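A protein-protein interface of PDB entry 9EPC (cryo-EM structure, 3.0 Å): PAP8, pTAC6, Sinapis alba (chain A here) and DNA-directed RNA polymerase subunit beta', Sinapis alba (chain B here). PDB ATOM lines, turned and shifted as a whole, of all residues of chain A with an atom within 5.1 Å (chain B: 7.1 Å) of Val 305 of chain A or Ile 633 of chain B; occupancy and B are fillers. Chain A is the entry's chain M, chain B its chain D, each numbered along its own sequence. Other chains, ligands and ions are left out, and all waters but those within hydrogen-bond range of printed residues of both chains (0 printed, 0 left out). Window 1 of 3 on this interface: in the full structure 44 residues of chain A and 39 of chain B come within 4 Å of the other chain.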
ATOM      1  N   ARG A 285      -9.287 -14.510 -29.487  1.00  0.00           N
ATOM      2  CA  ARG A 285     -10.681 -14.688 -29.858  1.00  0.00           C
ATOM      3  C   ARG A 285     -10.750 -15.154 -31.304  1.00  0.00           C
ATOM      4  O   ARG A 285      -9.762 -15.106 -32.041  1.00  0.00           O
ATOM      5  CB  ARG A 285     -11.470 -13.394 -29.654  1.00  0.00           C
ATOM      6  CG  ARG A 285     -12.877 -13.605 -29.153  1.00  0.00           C
ATOM      7  CD  ARG A 285     -13.570 -12.288 -28.884  1.00  0.00           C
ATOM      8  NE  ARG A 285     -14.822 -12.489 -28.166  1.00  0.00           N
ATOM      9  CZ  ARG A 285     -15.972 -12.804 -28.743  1.00  0.00           C
ATOM     10  NH1 ARG A 285     -16.070 -12.950 -30.054  1.00  0.00           N
ATOM     11  NH2 ARG A 285     -17.051 -12.980 -27.985  1.00  0.00           N
ATOM     12  N   ASP A 300     -13.163  -8.170 -19.194  1.00  0.00           N
ATOM     13  CA  ASP A 300     -14.567  -8.540 -19.129  1.00  0.00           C
ATOM     14  C   ASP A 300     -14.764  -9.716 -18.185  1.00  0.00           C
ATOM     15  O   ASP A 300     -13.939 -10.631 -18.126  1.00  0.00           O
ATOM     16  CB  ASP A 300     -15.094  -8.893 -20.517  1.00  0.00           C
ATOM     17  CG  ASP A 300     -15.129  -7.701 -21.446  1.00  0.00           C
ATOM     18  OD1 ASP A 300     -14.729  -6.600 -21.016  1.00  0.00           O
ATOM     19  OD2 ASP A 300     -15.561  -7.864 -22.606  1.00  0.00           O
ATOM     20  N   ASP A 301     -15.861  -9.679 -17.442  1.00  0.00           N
ATOM     21  CA  ASP A 301     -16.208 -10.795 -16.579  1.00  0.00           C
ATOM     22  C   ASP A 301     -16.462 -12.036 -17.430  1.00  0.00           C
ATOM     23  O   ASP A 301     -17.045 -11.932 -18.515  1.00  0.00           O
ATOM     24  CB  ASP A 301     -17.447 -10.446 -15.751  1.00  0.00           C
ATOM     25  CG  ASP A 301     -17.750 -11.471 -14.677  1.00  0.00           C
ATOM     26  OD1 ASP A 301     -18.059 -12.632 -15.016  1.00  0.00           O
ATOM     27  OD2 ASP A 301     -17.686 -11.113 -13.483  1.00  0.00           O
ATOM     28  N   PRO A 302     -16.024 -13.216 -16.987  1.00  0.00           N
ATOM     29  CA  PRO A 302     -16.315 -14.432 -17.760  1.00  0.00           C
ATOM     30  C   PRO A 302     -17.798 -14.663 -17.980  1.00  0.00           C
ATOM     31  O   PRO A 302     -18.181 -15.199 -19.026  1.00  0.00           O
ATOM     32  CB  PRO A 302     -15.684 -15.547 -16.912  1.00  0.00           C
ATOM     33  CG  PRO A 302     -15.435 -14.935 -15.572  1.00  0.00           C
ATOM     34  CD  PRO A 302     -15.157 -13.497 -15.834  1.00  0.00           C
ATOM     35  N   THR A 303     -18.646 -14.275 -17.027  1.00  0.00           N
ATOM     36  CA  THR A 303     -20.085 -14.348 -17.255  1.00  0.00           C
ATOM     37  C   THR A 303     -20.500 -13.440 -18.403  1.00  0.00           C
ATOM     38  O   THR A 303     -21.314 -13.828 -19.250  1.00  0.00           O
ATOM     39  CB  THR A 303     -20.839 -13.973 -15.981  1.00  0.00           C
ATOM     40  OG1 THR A 303     -20.662 -15.001 -15.001  1.00  0.00           O
ATOM     41  CG2 THR A 303     -22.316 -13.801 -16.267  1.00  0.00           C
ATOM     42  N   THR A 304     -19.943 -12.230 -18.453  1.00  0.00           N
ATOM     43  CA  THR A 304     -20.271 -11.308 -19.535  1.00  0.00           C
ATOM     44  C   THR A 304     -19.839 -11.864 -20.883  1.00  0.00           C
ATOM     45  O   THR A 304     -20.567 -11.743 -21.874  1.00  0.00           O
ATOM     46  CB  THR A 304     -19.615  -9.952 -19.281  1.00  0.00           C
ATOM     47  OG1 THR A 304     -20.064  -9.434 -18.024  1.00  0.00           O
ATOM     48  CG2 THR A 304     -19.981  -8.975 -20.377  1.00  0.00           C
ATOM     49  N   VAL A 305     -18.661 -12.487 -20.939  1.00  0.00           N
ATOM     50  CA  VAL A 305     -18.167 -13.033 -22.198  1.00  0.00           C
ATOM     51  C   VAL A 305     -19.102 -14.117 -22.716  1.00  0.00           C
ATOM     52  O   VAL A 305     -19.407 -14.175 -23.913  1.00  0.00           O
ATOM     53  CB  VAL A 305     -16.733 -13.562 -22.023  1.00  0.00           C
ATOM     54  CG1 VAL A 305     -16.241 -14.189 -23.308  1.00  0.00           C
ATOM     55  CG2 VAL A 305     -15.812 -12.441 -21.591  1.00  0.00           C
ATOM     56  N   ILE A 306     -19.570 -14.992 -21.827  1.00  0.00           N
ATOM     57  CA  ILE A 306     -20.467 -16.065 -22.245  1.00  0.00           C
ATOM     58  C   ILE A 306     -21.817 -15.499 -22.666  1.00  0.00           C
ATOM     59  O   ILE A 306     -22.359 -15.864 -23.715  1.00  0.00           O
ATOM     60  CB  ILE A 306     -20.616 -17.103 -21.122  1.00  0.00           C
ATOM     61  CG1 ILE A 306     -19.274 -17.779 -20.848  1.00  0.00           C
ATOM     62  CG2 ILE A 306     -21.663 -18.134 -21.490  1.00  0.00           C
ATOM     63  CD1 ILE A 306     -19.331 -18.829 -19.775  1.00  0.00           C
ATOM     64  N   GLU A 307     -22.380 -14.600 -21.856  1.00  0.00           N
ATOM     65  CA  GLU A 307     -23.687 -14.033 -22.172  1.00  0.00           C
ATOM     66  C   GLU A 307     -23.640 -13.221 -23.458  1.00  0.00           C
ATOM     67  O   GLU A 307     -24.589 -13.240 -24.249  1.00  0.00           O
ATOM     68  CB  GLU A 307     -24.183 -13.169 -21.016  1.00  0.00           C
ATOM     69  CG  GLU A 307     -24.649 -13.951 -19.804  1.00  0.00           C
ATOM     70  CD  GLU A 307     -25.219 -13.055 -18.720  1.00  0.00           C
ATOM     71  OE1 GLU A 307     -24.890 -11.850 -18.711  1.00  0.00           O
ATOM     72  OE2 GLU A 307     -25.998 -13.552 -17.883  1.00  0.00           O
ATOM     73  N   ARG A 308     -22.547 -12.490 -23.677  1.00  0.00           N
ATOM     74  CA  ARG A 308     -22.417 -11.689 -24.887  1.00  0.00           C
ATOM     75  C   ARG A 308     -22.441 -12.561 -26.134  1.00  0.00           C
ATOM     76  O   ARG A 308     -23.092 -12.220 -27.127  1.00  0.00           O
ATOM     77  CB  ARG A 308     -21.129 -10.875 -24.826  1.00  0.00           C
ATOM     78  CG  ARG A 308     -20.898  -9.956 -25.997  1.00  0.00           C
ATOM     79  CD  ARG A 308     -19.567  -9.255 -25.835  1.00  0.00           C
ATOM     80  NE  ARG A 308     -19.468  -8.591 -24.541  1.00  0.00           N
ATOM     81  CZ  ARG A 308     -18.341  -8.120 -24.026  1.00  0.00           C
ATOM     82  NH1 ARG A 308     -17.187  -8.243 -24.659  1.00  0.00           N
ATOM     83  NH2 ARG A 308     -18.373  -7.510 -22.846  1.00  0.00           N
ATOM     84  N   GLU A 309     -21.731 -13.688 -26.105  1.00  0.00           N
ATOM     85  CA  GLU A 309     -21.726 -14.583 -27.254  1.00  0.00           C
ATOM     86  C   GLU A 309     -23.073 -15.273 -27.424  1.00  0.00           C
ATOM     87  O   GLU A 309     -23.519 -15.508 -28.551  1.00  0.00           O
ATOM     88  CB  GLU A 309     -20.607 -15.612 -27.115  1.00  0.00           C
ATOM     89  CG  GLU A 309     -20.224 -16.285 -28.422  1.00  0.00           C
ATOM     90  CD  GLU A 309     -19.248 -15.465 -29.253  1.00  0.00           C
ATOM     91  OE1 GLU A 309     -18.327 -16.063 -29.846  1.00  0.00           O
ATOM     92  OE2 GLU A 309     -19.394 -14.226 -29.313  1.00  0.00           O
ATOM     93  N   PRO B 557     -25.193  -7.389 -23.717  1.00  0.00           N
ATOM     94  CA  PRO B 557     -24.150  -7.006 -22.756  1.00  0.00           C
ATOM     95  C   PRO B 557     -23.037  -6.176 -23.367  1.00  0.00           C
ATOM     96  O   PRO B 557     -22.482  -5.310 -22.680  1.00  0.00           O
ATOM     97  CB  PRO B 557     -23.634  -8.357 -22.249  1.00  0.00           C
ATOM     98  CG  PRO B 557     -24.776  -9.283 -22.438  1.00  0.00           C
ATOM     99  CD  PRO B 557     -25.462  -8.836 -23.692  1.00  0.00           C
ATOM    100  N   TRP B 603     -21.552 -20.344 -10.816  1.00  0.00           N
ATOM    101  CA  TRP B 603     -20.249 -20.931 -11.088  1.00  0.00           C
ATOM    102  C   TRP B 603     -19.879 -21.874  -9.956  1.00  0.00           C
ATOM    103  O   TRP B 603     -19.899 -21.482  -8.784  1.00  0.00           O
ATOM    104  CB  TRP B 603     -19.182 -19.851 -11.246  1.00  0.00           C
ATOM    105  CG  TRP B 603     -19.372 -19.017 -12.460  1.00  0.00           C
ATOM    106  CD1 TRP B 603     -20.104 -17.874 -12.561  1.00  0.00           C
ATOM    107  CD2 TRP B 603     -18.823 -19.258 -13.756  1.00  0.00           C
ATOM    108  NE1 TRP B 603     -20.044 -17.386 -13.841  1.00  0.00           N
ATOM    109  CE2 TRP B 603     -19.262 -18.219 -14.596  1.00  0.00           C
ATOM    110  CE3 TRP B 603     -18.001 -20.252 -14.289  1.00  0.00           C
ATOM    111  CZ2 TRP B 603     -18.907 -18.146 -15.936  1.00  0.00           C
ATOM    112  CZ3 TRP B 603     -17.650 -20.177 -15.620  1.00  0.00           C
ATOM    113  CH2 TRP B 603     -18.100 -19.132 -16.428  1.00  0.00           C
ATOM    114  N   VAL B 618     -13.473 -24.559 -29.323  1.00  0.00           N
ATOM    115  CA  VAL B 618     -12.347 -23.779 -28.823  1.00  0.00           C
ATOM    116  C   VAL B 618     -12.892 -22.740 -27.852  1.00  0.00           C
ATOM    117  O   VAL B 618     -14.090 -22.426 -27.901  1.00  0.00           O
ATOM    118  CB  VAL B 618     -11.569 -23.128 -29.978  1.00  0.00           C
ATOM    119  CG1 VAL B 618     -10.837 -24.185 -30.779  1.00  0.00           C
ATOM    120  CG2 VAL B 618     -12.513 -22.345 -30.870  1.00  0.00           C
ATOM    121  N   PRO B 619     -12.077 -22.204 -26.946  1.00  0.00           N
ATOM    122  CA  PRO B 619     -12.590 -21.209 -25.999  1.00  0.00           C
ATOM    123  C   PRO B 619     -13.180 -20.009 -26.721  1.00  0.00           C
ATOM    124  O   PRO B 619     -12.680 -19.576 -27.760  1.00  0.00           O
ATOM    125  CB  PRO B 619     -11.351 -20.817 -25.191  1.00  0.00           C
ATOM    126  CG  PRO B 619     -10.437 -21.963 -25.317  1.00  0.00           C
ATOM    127  CD  PRO B 619     -10.671 -22.544 -26.673  1.00  0.00           C
ATOM    128  N   ILE B 620     -14.267 -19.480 -26.158  1.00  0.00           N
ATOM    129  CA  ILE B 620     -14.869 -18.268 -26.702  1.00  0.00           C
ATOM    130  C   ILE B 620     -13.871 -17.123 -26.660  1.00  0.00           C
ATOM    131  O   ILE B 620     -13.765 -16.333 -27.605  1.00  0.00           O
ATOM    132  CB  ILE B 620     -16.154 -17.917 -25.934  1.00  0.00           C
ATOM    133  CG1 ILE B 620     -17.191 -19.026 -26.085  1.00  0.00           C
ATOM    134  CG2 ILE B 620     -16.717 -16.597 -26.414  1.00  0.00           C
ATOM    135  CD1 ILE B 620     -18.469 -18.754 -25.334  1.00  0.00           C
ATOM    136  N   GLU B 621     -13.115 -17.025 -25.571  1.00  0.00           N
ATOM    137  CA  GLU B 621     -12.193 -15.921 -25.371  1.00  0.00           C
ATOM    138  C   GLU B 621     -11.181 -16.328 -24.316  1.00  0.00           C
ATOM    139  O   GLU B 621     -11.543 -16.938 -23.308  1.00  0.00           O
ATOM    140  CB  GLU B 621     -12.949 -14.660 -24.947  1.00  0.00           C
ATOM    141  CG  GLU B 621     -12.083 -13.459 -24.663  1.00  0.00           C
ATOM    142  CD  GLU B 621     -12.902 -12.203 -24.461  1.00  0.00           C
ATOM    143  OE1 GLU B 621     -14.019 -12.127 -25.015  1.00  0.00           O
ATOM    144  OE2 GLU B 621     -12.438 -11.295 -23.742  1.00  0.00           O
ATOM    145  N   VAL B 622      -9.916 -15.999 -24.555  1.00  0.00           N
ATOM    146  CA  VAL B 622      -8.830 -16.321 -23.638  1.00  0.00           C
ATOM    147  C   VAL B 622      -8.246 -15.017 -23.120  1.00  0.00           C
ATOM    148  O   VAL B 622      -7.739 -14.205 -23.901  1.00  0.00           O
ATOM    149  CB  VAL B 622      -7.748 -17.175 -24.312  1.00  0.00           C
ATOM    150  CG1 VAL B 622      -6.636 -17.480 -23.331  1.00  0.00           C
ATOM    151  CG2 VAL B 622      -8.350 -18.454 -24.851  1.00  0.00           C
ATOM    152  N   HIS B 623      -8.310 -14.821 -21.807  1.00  0.00           N
ATOM    153  CA  HIS B 623      -7.769 -13.629 -21.158  1.00  0.00           C
ATOM    154  C   HIS B 623      -6.366 -13.962 -20.672  1.00  0.00           C
ATOM    155  O   HIS B 623      -6.186 -14.518 -19.588  1.00  0.00           O
ATOM    156  CB  HIS B 623      -8.667 -13.176 -20.016  1.00  0.00           C
ATOM    157  CG  HIS B 623     -10.013 -12.705 -20.462  1.00  0.00           C
ATOM    158  ND1 HIS B 623     -11.081 -12.579 -19.602  1.00  0.00           N
ATOM    159  CD2 HIS B 623     -10.463 -12.327 -21.680  1.00  0.00           C
ATOM    160  CE1 HIS B 623     -12.132 -12.144 -20.271  1.00  0.00           C
ATOM    161  NE2 HIS B 623     -11.786 -11.984 -21.535  1.00  0.00           N
ATOM    162  N   HIS B 631      -6.837 -17.144 -18.519  1.00  0.00           N
ATOM    163  CA  HIS B 631      -8.153 -17.728 -18.327  1.00  0.00           C
ATOM    164  C   HIS B 631      -8.733 -18.102 -19.681  1.00  0.00           C
ATOM    165  O   HIS B 631      -8.645 -17.330 -20.637  1.00  0.00           O
ATOM    166  CB  HIS B 631      -9.093 -16.752 -17.619  1.00  0.00           C
ATOM    167  CG  HIS B 631      -8.564 -16.233 -16.319  1.00  0.00           C
ATOM    168  ND1 HIS B 631      -7.386 -15.526 -16.223  1.00  0.00           N
ATOM    169  CD2 HIS B 631      -9.061 -16.308 -15.063  1.00  0.00           C
ATOM    170  CE1 HIS B 631      -7.176 -15.194 -14.962  1.00  0.00           C
ATOM    171  NE2 HIS B 631      -8.179 -15.658 -14.238  1.00  0.00           N
ATOM    172  N   GLU B 632      -9.320 -19.286 -19.759  1.00  0.00           N
ATOM    173  CA  GLU B 632      -9.957 -19.765 -20.978  1.00  0.00           C
ATOM    174  C   GLU B 632     -11.455 -19.842 -20.725  1.00  0.00           C
ATOM    175  O   GLU B 632     -11.917 -20.692 -19.959  1.00  0.00           O
ATOM    176  CB  GLU B 632      -9.394 -21.121 -21.392  1.00  0.00           C
ATOM    177  CG  GLU B 632      -7.923 -21.085 -21.747  1.00  0.00           C
ATOM    178  CD  GLU B 632      -7.384 -22.444 -22.133  1.00  0.00           C
ATOM    179  OE1 GLU B 632      -7.974 -23.460 -21.711  1.00  0.00           O
ATOM    180  OE2 GLU B 632      -6.373 -22.499 -22.864  1.00  0.00           O
ATOM    181  N   ILE B 633     -12.207 -18.951 -21.358  1.00  0.00           N
ATOM    182  CA  ILE B 633     -13.656 -18.913 -21.208  1.00  0.00           C
ATOM    183  C   ILE B 633     -14.258 -19.801 -22.287  1.00  0.00           C
ATOM    184  O   ILE B 633     -14.220 -19.466 -23.473  1.00  0.00           O
ATOM    185  CB  ILE B 633     -14.201 -17.484 -21.299  1.00  0.00           C
ATOM    186  CG1 ILE B 633     -13.750 -16.650 -20.099  1.00  0.00           C
ATOM    187  CG2 ILE B 633     -15.709 -17.504 -21.369  1.00  0.00           C
ATOM    188  CD1 ILE B 633     -12.480 -15.876 -20.330  1.00  0.00           C
ATOM    189  N   TYR B 634     -14.804 -20.940 -21.881  1.00  0.00           N
ATOM    190  CA  TYR B 634     -15.508 -21.809 -22.803  1.00  0.00           C
ATOM    191  C   TYR B 634     -16.997 -21.480 -22.774  1.00  0.00           C
ATOM    192  O   TYR B 634     -17.448 -20.578 -22.066  1.00  0.00           O
ATOM    193  CB  TYR B 634     -15.253 -23.274 -22.460  1.00  0.00           C
ATOM    194  CG  TYR B 634     -13.845 -23.724 -22.745  1.00  0.00           C
ATOM    195  CD1 TYR B 634     -12.819 -23.466 -21.851  1.00  0.00           C
ATOM    196  CD2 TYR B 634     -13.540 -24.411 -23.908  1.00  0.00           C
ATOM    197  CE1 TYR B 634     -11.531 -23.876 -22.109  1.00  0.00           C
ATOM    198  CE2 TYR B 634     -12.255 -24.824 -24.174  1.00  0.00           C
ATOM    199  CZ  TYR B 634     -11.255 -24.554 -23.271  1.00  0.00           C
ATOM    200  OH  TYR B 634      -9.971 -24.965 -23.533  1.00  0.00           O
ATOM    201  N   ALA B 635     -17.777 -22.221 -23.560  1.00  0.00           N
ATOM    202  CA  ALA B 635     -19.209 -21.961 -23.610  1.00  0.00           C
ATOM    203  C   ALA B 635     -19.895 -22.316 -22.299  1.00  0.00           C
ATOM    204  O   ALA B 635     -20.956 -21.763 -21.989  1.00  0.00           O
ATOM    205  CB  ALA B 635     -19.842 -22.734 -24.766  1.00  0.00           C
ATOM    206  N   HIS B 636     -19.311 -23.222 -21.516  1.00  0.00           N
ATOM    207  CA  HIS B 636     -19.955 -23.707 -20.308  1.00  0.00           C
ATOM    208  C   HIS B 636     -19.061 -23.734 -19.081  1.00  0.00           C
ATOM    209  O   HIS B 636     -19.567 -24.006 -17.988  1.00  0.00           O
ATOM    210  CB  HIS B 636     -20.513 -25.119 -20.532  1.00  0.00           C
ATOM    211  CG  HIS B 636     -21.526 -25.197 -21.629  1.00  0.00           C
ATOM    212  ND1 HIS B 636     -22.867 -24.961 -21.419  1.00  0.00           N
ATOM    213  CD2 HIS B 636     -21.394 -25.474 -22.946  1.00  0.00           C
ATOM    214  CE1 HIS B 636     -23.518 -25.095 -22.560  1.00  0.00           C
ATOM    215  NE2 HIS B 636     -22.648 -25.406 -23.502  1.00  0.00           N
ATOM    216  N   TYR B 637     -17.764 -23.469 -19.210  1.00  0.00           N
ATOM    217  CA  TYR B 637     -16.888 -23.504 -18.052  1.00  0.00           C
ATOM    218  C   TYR B 637     -15.702 -22.583 -18.273  1.00  0.00           C
ATOM    219  O   TYR B 637     -15.360 -22.231 -19.404  1.00  0.00           O
ATOM    220  CB  TYR B 637     -16.411 -24.928 -17.747  1.00  0.00           C
ATOM    221  CG  TYR B 637     -15.972 -25.708 -18.959  1.00  0.00           C
ATOM    222  CD1 TYR B 637     -14.675 -25.618 -19.433  1.00  0.00           C
ATOM    223  CD2 TYR B 637     -16.855 -26.542 -19.625  1.00  0.00           C
ATOM    224  CE1 TYR B 637     -14.271 -26.331 -20.538  1.00  0.00           C
ATOM    225  CE2 TYR B 637     -16.461 -27.259 -20.732  1.00  0.00           C
ATOM    226  CZ  TYR B 637     -15.168 -27.149 -21.184  1.00  0.00           C
ATOM    227  OH  TYR B 637     -14.768 -27.864 -22.289  1.00  0.00           O
ATOM    228  N   LEU B 638     -15.078 -22.195 -17.166  1.00  0.00           N
ATOM    229  CA  LEU B 638     -13.894 -21.350 -17.165  1.00  0.00           C
ATOM    230  C   LEU B 638     -12.730 -22.147 -16.603  1.00  0.00           C
ATOM    231  O   LEU B 638     -12.856 -22.777 -15.550  1.00  0.00           O
ATOM    232  CB  LEU B 638     -14.122 -20.089 -16.333  1.00  0.00           C
ATOM    233  CG  LEU B 638     -12.872 -19.332 -15.889  1.00  0.00           C
ATOM    234  CD1 LEU B 638     -12.214 -18.646 -17.066  1.00  0.00           C
ATOM    235  CD2 LEU B 638     -13.215 -18.331 -14.808  1.00  0.00           C
ATOM    236  N   ILE B 639     -11.602 -22.119 -17.306  1.00  0.00           N
ATOM    237  CA  ILE B 639     -10.401 -22.834 -16.899  1.00  0.00           C
ATOM    238  C   ILE B 639      -9.278 -21.826 -16.729  1.00  0.00           C
ATOM    239  O   ILE B 639      -8.984 -21.059 -17.651  1.00  0.00           O
ATOM    240  CB  ILE B 639     -10.017 -23.919 -17.916  1.00  0.00           C
ATOM    241  CG1 ILE B 639     -11.114 -24.977 -17.977  1.00  0.00           C
ATOM    242  CG2 ILE B 639      -8.693 -24.546 -17.543  1.00  0.00           C
ATOM    243  CD1 ILE B 639     -10.877 -26.029 -19.009  1.00  0.00           C
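Ile 620 of chain B touches Arg 285 of chain A.
O of Asp 300 of chain A touches CE1 of His 623 of chain B, at 3.2 Å.
CB of Pro 302 of chain A touches CG1 of Ile 633 of chain B, at 3.9 Å.
CG1 of Val 305 of chain A touches OE1 of Glu 621 of chain B (3.5 Å).
CE1 of His 623 of chain B touches CG2 of Val 305 of chain A, 3.9 Å away.
CG2 of Ile 633 of chain B touches CG1 of Val 305 of chain A, 3.9 Å away.
Trp 603 of chain B touches Ile 306 of chain A (CH2 to CD1, 3.6 Å).
CG2 of Ile 633 of chain B touches CG1 of Ile 306 of chain A, at 3.6 Å.
Ile 306 of chain A touches Tyr 634 of chain B (CD1 to O, 3.4 Å).
CG2 of Ile 620 of chain B touches OE1 of Glu 309 of chain A, 3.8 Å away.
The side-chain carboxylate of Glu 632 of chain B is in hydrogen-bond range of the side-chain hydroxyl of Tyr 634 of chain B, 3.1 Å away.
N of Thr 303 of chain A lies within hydrogen-bond range of OD1 of Asp 301 of chain A (2.7 Å).
NH1 of Arg 308 of chain A is in salt-bridge range of OD2 of Asp 300 of chain A (2.6 Å).
OE2 of Glu 621 of chain B lies within hydrogen-bond range of NE2 of His 623 of chain B.
N of Ile 620 of chain B lies within hydrogen-bond range of O of Ile 633 of chain B (2.7 Å).
The backbone carbonyl oxygen of Glu 621 of chain B lies within hydrogen-bond range of the backbone NH of Ile 633 of chain B.
Val 305 of chain A touches four residues of chain B.
Ile 633 of chain B touches three residues of chain A.
Printed residues of chain B within 4 Å of Asp 300 of chain A: His 623 (3.2 Å).
Printed residues of chain B within 4 Å of Thr 303 of chain A: Trp 603 (2.7 Å).
Arg 308 of chain A touches none of the printed residues of chain B.
Asp 301 of chain A touches none of the printed residues of chain B.
The nearest printed residue of chain B that does not touch Val 305 of chain A is Pro 557 of chain B (6.6 Å).
The nearest printed residue of chain B that does not touch Pro 302 of chain A is Leu 638 of chain B (4.1 Å).
Of the 17 printed residues of chain B, 7 touch a printed residue of chain A.
Hydrophobic or aromatic side chains of chain B that line the printed part of chain A: Trp 603, Ile 620, His 623 and Ile 633.
Printed residues of chain A that touch a printed residue of chain B: Arg 285, Asp 300, Pro 302, Thr 303, Val 305, Ile 306 and Glu 309.
NE of Arg 285 of chain A is in salt-bridge range of OE1 of Glu 621 of chain B, 3.3 Å away.
The indole nitrogen of Trp 603 of chain B is in hydrogen-bond range of the side-chain hydroxyl of Thr 303 of chain A.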
